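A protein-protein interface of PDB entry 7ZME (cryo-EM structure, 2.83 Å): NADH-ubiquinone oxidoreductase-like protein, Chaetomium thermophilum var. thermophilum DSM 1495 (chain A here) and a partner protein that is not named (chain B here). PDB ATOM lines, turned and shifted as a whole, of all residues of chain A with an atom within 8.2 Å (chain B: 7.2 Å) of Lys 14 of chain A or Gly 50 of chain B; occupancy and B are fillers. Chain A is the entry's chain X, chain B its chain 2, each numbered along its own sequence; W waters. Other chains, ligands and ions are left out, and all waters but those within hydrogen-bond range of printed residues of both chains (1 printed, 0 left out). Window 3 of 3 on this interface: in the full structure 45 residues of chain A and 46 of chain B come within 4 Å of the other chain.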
ATOM      1  N   TYR A   9       8.210  -3.794  -4.068  1.00  0.00           N
ATOM      2  CA  TYR A   9       9.050  -3.349  -2.924  1.00  0.00           C
ATOM      3  C   TYR A   9       8.456  -2.010  -2.488  1.00  0.00           C
ATOM      4  O   TYR A   9       8.685  -1.025  -3.198  1.00  0.00           O
ATOM      5  CB  TYR A   9      10.496  -3.228  -3.397  1.00  0.00           C
ATOM      6  CG  TYR A   9      11.589  -3.203  -2.362  1.00  0.00           C
ATOM      7  CD1 TYR A   9      12.215  -4.369  -1.959  1.00  0.00           C
ATOM      8  CD2 TYR A   9      12.056  -2.006  -1.851  1.00  0.00           C
ATOM      9  CE1 TYR A   9      13.245  -4.352  -1.034  1.00  0.00           C
ATOM     10  CE2 TYR A   9      13.085  -1.969  -0.928  1.00  0.00           C
ATOM     11  CZ  TYR A   9      13.682  -3.147  -0.519  1.00  0.00           C
ATOM     12  OH  TYR A   9      14.701  -3.116   0.383  1.00  0.00           O
ATOM     13  N   PHE A  11       8.465  -0.770   0.948  1.00  0.00           N
ATOM     14  CA  PHE A  11       9.074  -0.230   2.176  1.00  0.00           C
ATOM     15  C   PHE A  11      10.578  -0.298   2.006  1.00  0.00           C
ATOM     16  O   PHE A  11      11.056  -1.226   1.357  1.00  0.00           O
ATOM     17  CB  PHE A  11       8.577  -1.034   3.380  1.00  0.00           C
ATOM     18  CG  PHE A  11       7.079  -1.110   3.501  1.00  0.00           C
ATOM     19  CD1 PHE A  11       6.360  -0.054   4.033  1.00  0.00           C
ATOM     20  CD2 PHE A  11       6.389  -2.231   3.072  1.00  0.00           C
ATOM     21  CE1 PHE A  11       4.981  -0.120   4.138  1.00  0.00           C
ATOM     22  CE2 PHE A  11       5.010  -2.296   3.179  1.00  0.00           C
ATOM     23  CZ  PHE A  11       4.310  -1.242   3.712  1.00  0.00           C
ATOM     24  N   PRO A  12      11.334   0.650   2.584  1.00  0.00           N
ATOM     25  CA  PRO A  12      12.782   0.610   2.505  1.00  0.00           C
ATOM     26  C   PRO A  12      13.351  -0.389   3.522  1.00  0.00           C
ATOM     27  O   PRO A  12      13.118  -0.235   4.684  1.00  0.00           O
ATOM     28  CB  PRO A  12      13.135   2.083   2.754  1.00  0.00           C
ATOM     29  CG  PRO A  12      12.058   2.596   3.678  1.00  0.00           C
ATOM     30  CD  PRO A  12      10.817   1.831   3.278  1.00  0.00           C
ATOM     31  N   SER A  13      14.119  -1.364   3.046  1.00  0.00           N
ATOM     32  CA  SER A  13      14.631  -2.439   3.936  1.00  0.00           C
ATOM     33  C   SER A  13      16.138  -2.327   4.097  1.00  0.00           C
ATOM     34  O   SER A  13      16.745  -1.578   3.339  1.00  0.00           O
ATOM     35  CB  SER A  13      14.248  -3.786   3.405  1.00  0.00           C
ATOM     36  OG  SER A  13      12.875  -3.807   3.054  1.00  0.00           O
ATOM     37  N   LYS A  14      16.704  -3.071   5.041  1.00  0.00           N
ATOM     38  CA  LYS A  14      18.174  -3.078   5.244  1.00  0.00           C
ATOM     39  C   LYS A  14      18.755  -4.281   4.516  1.00  0.00           C
ATOM     40  O   LYS A  14      18.280  -5.397   4.763  1.00  0.00           O
ATOM     41  CB  LYS A  14      18.513  -3.171   6.732  1.00  0.00           C
ATOM     42  CG  LYS A  14      19.989  -3.307   7.077  1.00  0.00           C
ATOM     43  CD  LYS A  14      20.805  -2.096   6.701  1.00  0.00           C
ATOM     44  CE  LYS A  14      22.265  -2.212   7.081  1.00  0.00           C
ATOM     45  NZ  LYS A  14      23.009  -0.983   6.721  1.00  0.00           N
ATOM     46  N   THR A  15      19.803  -4.044   3.725  1.00  0.00           N
ATOM     47  CA  THR A  15      20.518  -5.133   3.028  1.00  0.00           C
ATOM     48  C   THR A  15      21.649  -5.581   3.949  1.00  0.00           C
ATOM     49  O   THR A  15      22.431  -4.725   4.385  1.00  0.00           O
ATOM     50  CB  THR A  15      21.046  -4.641   1.675  1.00  0.00           C
ATOM     51  OG1 THR A  15      19.915  -4.409   0.837  1.00  0.00           O
ATOM     52  CG2 THR A  15      21.996  -5.612   1.011  1.00  0.00           C
ATOM     53  N   VAL A  16      21.702  -6.868   4.254  1.00  0.00           N
ATOM     54  CA  VAL A  16      22.810  -7.418   5.082  1.00  0.00           C
ATOM     55  C   VAL A  16      23.647  -8.305   4.159  1.00  0.00           C
ATOM     56  O   VAL A  16      23.053  -8.995   3.313  1.00  0.00           O
ATOM     57  CB  VAL A  16      22.258  -8.198   6.290  1.00  0.00           C
ATOM     58  CG1 VAL A  16      23.365  -8.650   7.225  1.00  0.00           C
ATOM     59  CG2 VAL A  16      21.199  -7.406   7.038  1.00  0.00           C
ATOM     60  N   LYS A  17      24.974  -8.249   4.281  1.00  0.00           N
ATOM     61  CA  LYS A  17      25.816  -9.168   3.477  1.00  0.00           C
ATOM     62  C   LYS A  17      25.723 -10.563   4.097  1.00  0.00           C
ATOM     63  O   LYS A  17      26.152 -10.720   5.244  1.00  0.00           O
ATOM     64  CB  LYS A  17      27.255  -8.660   3.427  1.00  0.00           C
ATOM     65  CG  LYS A  17      28.250  -9.556   2.700  1.00  0.00           C
ATOM     66  CD  LYS A  17      28.233  -9.377   1.200  1.00  0.00           C
ATOM     67  CE  LYS A  17      29.392 -10.069   0.515  1.00  0.00           C
ATOM     68  NZ  LYS A  17      29.516  -9.659  -0.904  1.00  0.00           N
ATOM     69  N   LEU A  22      18.012 -14.324   0.706  1.00  0.00           N
ATOM     70  CA  LEU A  22      17.127 -13.891   1.811  1.00  0.00           C
ATOM     71  C   LEU A  22      15.698 -14.258   1.401  1.00  0.00           C
ATOM     72  O   LEU A  22      15.285 -13.871   0.302  1.00  0.00           O
ATOM     73  CB  LEU A  22      17.287 -12.383   2.033  1.00  0.00           C
ATOM     74  CG  LEU A  22      16.138 -11.687   2.770  1.00  0.00           C
ATOM     75  CD1 LEU A  22      16.177 -11.976   4.261  1.00  0.00           C
ATOM     76  CD2 LEU A  22      16.157 -10.187   2.527  1.00  0.00           C
ATOM     77  N   ASN A  25      12.917 -11.417   6.060  1.00  0.00           N
ATOM     78  CA  ASN A  25      13.726 -10.743   7.104  1.00  0.00           C
ATOM     79  C   ASN A  25      12.899 -10.787   8.383  1.00  0.00           C
ATOM     80  O   ASN A  25      13.483 -10.642   9.463  1.00  0.00           O
ATOM     81  CB  ASN A  25      14.242  -9.368   6.660  1.00  0.00           C
ATOM     82  CG  ASN A  25      13.246  -8.228   6.694  1.00  0.00           C
ATOM     83  OD1 ASN A  25      12.064  -8.409   6.965  1.00  0.00           O
ATOM     84  ND2 ASN A  25      13.729  -7.030   6.413  1.00  0.00           N
ATOM     85  N   ARG A 144      12.177  -7.455  12.651  1.00  0.00           N
ATOM     86  CA  ARG A 144      13.025  -7.928  11.520  1.00  0.00           C
ATOM     87  C   ARG A 144      14.461  -8.160  12.005  1.00  0.00           C
ATOM     88  O   ARG A 144      14.993  -7.270  12.696  1.00  0.00           O
ATOM     89  CB  ARG A 144      12.879  -7.034  10.283  1.00  0.00           C
ATOM     90  CG  ARG A 144      13.280  -5.579  10.461  1.00  0.00           C
ATOM     91  CD  ARG A 144      14.647  -5.315   9.871  1.00  0.00           C
ATOM     92  NE  ARG A 144      15.161  -4.031  10.313  1.00  0.00           N
ATOM     93  CZ  ARG A 144      16.402  -3.624  10.110  1.00  0.00           C
ATOM     94  NH1 ARG A 144      17.248  -4.413   9.479  1.00  0.00           N
ATOM     95  NH2 ARG A 144      16.795  -2.441  10.537  1.00  0.00           N
ATOM     96  N   TYR A 145      15.056  -9.315  11.677  1.00  0.00           N
ATOM     97  CA  TYR A 145      16.437  -9.659  12.109  1.00  0.00           C
ATOM     98  C   TYR A 145      16.526  -9.735  13.635  1.00  0.00           C
ATOM     99  O   TYR A 145      17.632  -9.580  14.150  1.00  0.00           O
ATOM    100  CB  TYR A 145      17.487  -8.767  11.446  1.00  0.00           C
ATOM    101  CG  TYR A 145      17.567  -8.864   9.946  1.00  0.00           C
ATOM    102  CD1 TYR A 145      17.788 -10.074   9.312  1.00  0.00           C
ATOM    103  CD2 TYR A 145      17.450  -7.731   9.161  1.00  0.00           C
ATOM    104  CE1 TYR A 145      17.872 -10.158   7.933  1.00  0.00           C
ATOM    105  CE2 TYR A 145      17.529  -7.797   7.781  1.00  0.00           C
ATOM    106  CZ  TYR A 145      17.742  -9.015   7.166  1.00  0.00           C
ATOM    107  OH  TYR A 145      17.822  -9.075   5.807  1.00  0.00           O
ATOM    108  N   HIS A 164       8.518  -7.695   4.375  1.00  0.00           N
ATOM    109  CA  HIS A 164       9.493  -8.782   4.692  1.00  0.00           C
ATOM    110  C   HIS A 164      10.855  -8.592   4.023  1.00  0.00           C
ATOM    111  O   HIS A 164      11.621  -9.564   4.031  1.00  0.00           O
ATOM    112  CB  HIS A 164       8.853 -10.139   4.416  1.00  0.00           C
ATOM    113  CG  HIS A 164       7.601 -10.344   5.200  1.00  0.00           C
ATOM    114  ND1 HIS A 164       7.583 -11.013   6.401  1.00  0.00           N
ATOM    115  CD2 HIS A 164       6.341  -9.925   4.990  1.00  0.00           C
ATOM    116  CE1 HIS A 164       6.362 -11.031   6.878  1.00  0.00           C
ATOM    117  NE2 HIS A 164       5.586 -10.368   6.037  1.00  0.00           N
ATOM    118  N   GLY A 165      11.116  -7.434   3.412  1.00  0.00           N
ATOM    119  CA  GLY A 165      12.449  -7.131   2.859  1.00  0.00           C
ATOM    120  C   GLY A 165      12.721  -7.730   1.497  1.00  0.00           C
ATOM    121  O   GLY A 165      13.829  -7.515   0.990  1.00  0.00           O
ATOM    122  N   VAL A 166      11.818  -8.431   0.894  1.00  0.00           N
ATOM    123  CA  VAL A 166      12.085  -9.090  -0.417  1.00  0.00           C
ATOM    124  C   VAL A 166      11.140  -8.544  -1.485  1.00  0.00           C
ATOM    125  O   VAL A 166      10.011  -8.171  -1.133  1.00  0.00           O
ATOM    126  CB  VAL A 166      11.991 -10.626  -0.345  1.00  0.00           C
ATOM    127  CG1 VAL A 166      13.101 -11.232   0.491  1.00  0.00           C
ATOM    128  CG2 VAL A 166      10.633 -11.101   0.141  1.00  0.00           C
ATOM    129  N   PHE B  46      26.924 -13.061   9.290  1.00  0.00           N
ATOM    130  CA  PHE B  46      26.540 -11.908   8.445  1.00  0.00           C
ATOM    131  C   PHE B  46      27.738 -10.966   8.424  1.00  0.00           C
ATOM    132  O   PHE B  46      28.516 -11.022   9.388  1.00  0.00           O
ATOM    133  CB  PHE B  46      25.309 -11.203   9.027  1.00  0.00           C
ATOM    134  CG  PHE B  46      25.526 -10.373  10.268  1.00  0.00           C
ATOM    135  CD1 PHE B  46      25.890  -9.039  10.181  1.00  0.00           C
ATOM    136  CD2 PHE B  46      25.326 -10.913  11.527  1.00  0.00           C
ATOM    137  CE1 PHE B  46      26.085  -8.275  11.321  1.00  0.00           C
ATOM    138  CE2 PHE B  46      25.512 -10.144  12.667  1.00  0.00           C
ATOM    139  CZ  PHE B  46      25.891  -8.828  12.563  1.00  0.00           C
ATOM    140  N   ILE B  47      27.904 -10.169   7.369  1.00  0.00           N
ATOM    141  CA  ILE B  47      28.977  -9.136   7.401  1.00  0.00           C
ATOM    142  C   ILE B  47      28.277  -7.782   7.294  1.00  0.00           C
ATOM    143  O   ILE B  47      27.486  -7.612   6.352  1.00  0.00           O
ATOM    144  CB  ILE B  47      30.021  -9.356   6.295  1.00  0.00           C
ATOM    145  CG1 ILE B  47      30.718 -10.713   6.420  1.00  0.00           C
ATOM    146  CG2 ILE B  47      31.027  -8.215   6.274  1.00  0.00           C
ATOM    147  CD1 ILE B  47      31.657 -10.808   7.594  1.00  0.00           C
ATOM    148  N   SER B  48      28.537  -6.865   8.230  1.00  0.00           N
ATOM    149  CA  SER B  48      27.794  -5.578   8.240  1.00  0.00           C
ATOM    150  C   SER B  48      28.382  -4.605   9.252  1.00  0.00           C
ATOM    151  O   SER B  48      28.877  -5.070  10.288  1.00  0.00           O
ATOM    152  CB  SER B  48      26.324  -5.785   8.515  1.00  0.00           C
ATOM    153  OG  SER B  48      25.655  -4.550   8.714  1.00  0.00           O
ATOM    154  N   LYS B  49      28.313  -3.311   8.968  1.00  0.00           N
ATOM    155  CA  LYS B  49      28.707  -2.316   9.952  1.00  0.00           C
ATOM    156  C   LYS B  49      27.675  -2.143  11.053  1.00  0.00           C
ATOM    157  O   LYS B  49      27.964  -1.481  12.054  1.00  0.00           O
ATOM    158  CB  LYS B  49      28.946  -0.962   9.284  1.00  0.00           C
ATOM    159  CG  LYS B  49      30.242  -0.851   8.531  1.00  0.00           C
ATOM    160  CD  LYS B  49      30.595   0.606   8.327  1.00  0.00           C
ATOM    161  CE  LYS B  49      31.879   0.747   7.562  1.00  0.00           C
ATOM    162  NZ  LYS B  49      31.674   0.353   6.153  1.00  0.00           N
ATOM    163  N   GLY B  50      26.486  -2.711  10.891  1.00  0.00           N
ATOM    164  CA  GLY B  50      25.439  -2.542  11.871  1.00  0.00           C
ATOM    165  C   GLY B  50      24.052  -2.722  11.299  1.00  0.00           C
ATOM    166  O   GLY B  50      23.752  -2.247  10.202  1.00  0.00           O
ATOM    167  N   ILE B  51      23.194  -3.413  12.047  1.00  0.00           N
ATOM    168  CA  ILE B  51      21.781  -3.623  11.625  1.00  0.00           C
ATOM    169  C   ILE B  51      20.905  -3.110  12.762  1.00  0.00           C
ATOM    170  O   ILE B  51      21.007  -3.670  13.858  1.00  0.00           O
ATOM    171  CB  ILE B  51      21.511  -5.113  11.342  1.00  0.00           C
ATOM    172  CG1 ILE B  51      22.486  -5.696  10.318  1.00  0.00           C
ATOM    173  CG2 ILE B  51      20.064  -5.346  10.945  1.00  0.00           C
ATOM    174  CD1 ILE B  51      22.609  -7.193  10.397  1.00  0.00           C
ATOM    175  N   GLY B  52      20.102  -2.075  12.513  1.00  0.00           N
ATOM    176  CA  GLY B  52      19.179  -1.541  13.526  1.00  0.00           C
ATOM    177  C   GLY B  52      18.153  -2.580  13.921  1.00  0.00           C
ATOM    178  O   GLY B  52      17.667  -3.291  13.045  1.00  0.00           O
ATOM    179  N   HIS B  59      21.105  -2.133  17.986  1.00  0.00           N
ATOM    180  CA  HIS B  59      21.804  -2.540  16.778  1.00  0.00           C
ATOM    181  C   HIS B  59      22.697  -3.728  17.091  1.00  0.00           C
ATOM    182  O   HIS B  59      22.996  -4.021  18.250  1.00  0.00           O
ATOM    183  CB  HIS B  59      22.632  -1.393  16.176  1.00  0.00           C
ATOM    184  CG  HIS B  59      23.874  -1.072  16.945  1.00  0.00           C
ATOM    185  ND1 HIS B  59      25.128  -1.456  16.525  1.00  0.00           N
ATOM    186  CD2 HIS B  59      24.056  -0.406  18.108  1.00  0.00           C
ATOM    187  CE1 HIS B  59      26.029  -1.044  17.397  1.00  0.00           C
ATOM    188  NE2 HIS B  59      25.404  -0.404  18.368  1.00  0.00           N
ATOM    189  N   ILE B  60      23.003  -4.473  16.009  1.00  0.00           N
ATOM    190  CA  ILE B  60      23.931  -5.626  16.132  1.00  0.00           C
ATOM    191  C   ILE B  60      25.065  -5.435  15.135  1.00  0.00           C
ATOM    192  O   ILE B  60      24.788  -5.036  14.008  1.00  0.00           O
ATOM    193  CB  ILE B  60      23.205  -6.960  15.907  1.00  0.00           C
ATOM    194  CG1 ILE B  60      22.169  -6.844  14.791  1.00  0.00           C
ATOM    195  CG2 ILE B  60      22.601  -7.484  17.197  1.00  0.00           C
ATOM    196  CD1 ILE B  60      22.166  -8.015  13.859  1.00  0.00           C
ATOM    197  N   THR B  61      26.308  -5.697  15.574  1.00  0.00           N
ATOM    198  CA  THR B  61      27.497  -5.650  14.685  1.00  0.00           C
ATOM    199  C   THR B  61      28.279  -6.928  14.981  1.00  0.00           C
ATOM    200  O   THR B  61      27.994  -7.539  16.005  1.00  0.00           O
ATOM    201  CB  THR B  61      28.339  -4.398  14.943  1.00  0.00           C
ATOM    202  OG1 THR B  61      27.461  -3.275  14.989  1.00  0.00           O
ATOM    203  CG2 THR B  61      29.388  -4.155  13.882  1.00  0.00           C
ATOM    204  N   ASN B  62      29.190  -7.341  14.109  1.00  0.00           N
ATOM    205  CA  ASN B  62      30.054  -8.506  14.408  1.00  0.00           C
ATOM    206  C   ASN B  62      30.868  -8.143  15.649  1.00  0.00           C
ATOM    207  O   ASN B  62      31.072  -9.017  16.492  1.00  0.00           O
ATOM    208  CB  ASN B  62      30.914  -8.889  13.204  1.00  0.00           C
ATOM    209  CG  ASN B  62      30.113  -9.254  11.975  1.00  0.00           C
ATOM    210  OD1 ASN B  62      30.137  -8.534  10.981  1.00  0.00           O
ATOM    211  ND2 ASN B  62      29.406 -10.369  12.036  1.00  0.00           N
ATOM    212  N   GLU B 293      32.907   2.866  18.753  1.00  0.00           N
ATOM    213  CA  GLU B 293      32.174   3.086  17.493  1.00  0.00           C
ATOM    214  C   GLU B 293      31.717   4.539  17.454  1.00  0.00           C
ATOM    215  O   GLU B 293      31.541   5.086  16.368  1.00  0.00           O
ATOM    216  CB  GLU B 293      31.004   2.120  17.418  1.00  0.00           C
ATOM    217  CG  GLU B 293      30.650   1.703  16.004  1.00  0.00           C
ATOM    218  CD  GLU B 293      29.463   0.763  15.898  1.00  0.00           C
ATOM    219  OE1 GLU B 293      29.005   0.270  16.945  1.00  0.00           O
ATOM    220  OE2 GLU B 293      29.002   0.527  14.767  1.00  0.00           O
ATOM    221  N   TYR B 297      32.633   7.079  14.057  1.00  0.00           N
ATOM    222  CA  TYR B 297      31.659   7.810  13.213  1.00  0.00           C
ATOM    223  C   TYR B 297      31.867   9.328  13.320  1.00  0.00           C
ATOM    224  O   TYR B 297      31.705  10.010  12.303  1.00  0.00           O
ATOM    225  CB  TYR B 297      30.250   7.244  13.382  1.00  0.00           C
ATOM    226  CG  TYR B 297      30.056   5.867  12.808  1.00  0.00           C
ATOM    227  CD1 TYR B 297      29.889   5.679  11.447  1.00  0.00           C
ATOM    228  CD2 TYR B 297      30.035   4.750  13.622  1.00  0.00           C
ATOM    229  CE1 TYR B 297      29.713   4.417  10.908  1.00  0.00           C
ATOM    230  CE2 TYR B 297      29.861   3.482  13.101  1.00  0.00           C
ATOM    231  CZ  TYR B 297      29.699   3.313  11.740  1.00  0.00           C
ATOM    232  OH  TYR B 297      29.526   2.060  11.230  1.00  0.00           O
ATOM    233  N   ILE B 567      36.007  -4.500   8.662  1.00  0.00           N
ATOM    234  CA  ILE B 567      34.580  -4.265   8.447  1.00  0.00           C
ATOM    235  C   ILE B 567      34.197  -2.861   8.898  1.00  0.00           C
ATOM    236  O   ILE B 567      33.449  -2.154   8.213  1.00  0.00           O
ATOM    237  CB  ILE B 567      33.744  -5.338   9.166  1.00  0.00           C
ATOM    238  CG1 ILE B 567      34.029  -6.719   8.573  1.00  0.00           C
ATOM    239  CG2 ILE B 567      32.261  -5.009   9.093  1.00  0.00           C
ATOM    240  CD1 ILE B 567      33.548  -7.864   9.424  1.00  0.00           C
HETATM  241  O   HOH W   1      26.014  -1.820   7.148  1.00  0.00           O
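The backbone NH of Tyr 145 of chain A sits at hydrogen-bond distance from the backbone carbonyl oxygen of Asn 25 of chain A, at 3.0 Å. The backbone NH (N) of Ile 51 of chain B sits at hydrogen-bond distance from the backbone carbonyl oxygen (O) of Ile 60 of chain B (3.0 Å). ND2 of Asn 62 of chain B lies within hydrogen-bond range of O of Phe 46 of chain B (2.9 Å). The backbone NH (N) of Gly 50 of chain B is in hydrogen-bond range of the side-chain hydroxyl (OG) of Ser 48 of chain B.
Water W1 lies within hydrogen-bond range of NZ of Lys 14 of chain A (3.1 Å), OG of Ser 48 of chain B (3.2 Å) and N of Lys 49 of chain B (3.3 Å).
Among the printed residues, merely in contact across the chains: Lys 14 of chain A with Gly 50 of chain B (3.5 Å), Val 16 of chain A with Phe 46 of chain B (3.7 Å), Val 16 of chain A with Ile 51 of chain B (3.6 Å), Lys 17 of chain A with Phe 46 of chain B (3.4 Å), Arg 144 of chain A with Ile 51 of chain B (3.3 Å) and Tyr 145 of chain A with Ile 51 of chain B (3.96 Å).
The backbone carbonyl oxygen (O) of Lys 17 of chain A sits at hydrogen-bond distance from the backbone NH (N) of Ile 47 of chain B (2.8 Å). The guanidinium group of Arg 144 of chain A lies within hydrogen-bond range of the backbone carbonyl oxygen of Gly 52 of chain B (2.8 Å).
Hydrophobic or aromatic side chains of chain A that line the printed part of chain B: Val 16 and Tyr 145. Of the 14 printed residues of chain B, 5 touch a printed residue of chain A. Hydrophobic or aromatic side chains of chain B within 4 Å of the printed part of chain A: Phe 46 and Ile 51. Among the printed residues, no Asp or Glu carboxylate lies within 4 Å of a Lys or Arg side-chain nitrogen of the other chain.
Of chain B, only Gly 50 comes within 4 Å of Lys 14 of chain A. Printed residues of chain A within 4 Å of Gly 50 of chain B: Lys 14 (3.5 Å). Printed residues of chain B within 4 Å of Val 16 of chain A: Phe 46 (3.7 Å) and Ile 51 (3.6 Å). Printed residues of chain B within 4 Å of Arg 144 of chain A: Ile 51 (3.3 Å) and Gly 52 (2.8 Å). Of the printed residues of chain A, Phe 46 of chain B touches Val 16 (3.7 Å) and Lys 17 (3.4 Å). Of the printed residues of chain A, Ile 47 of chain B touches Lys 17. Phe 11 of chain A touches none of the printed residues of chain B. Thr 15 of chain A touches none of the printed residues of chain B.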
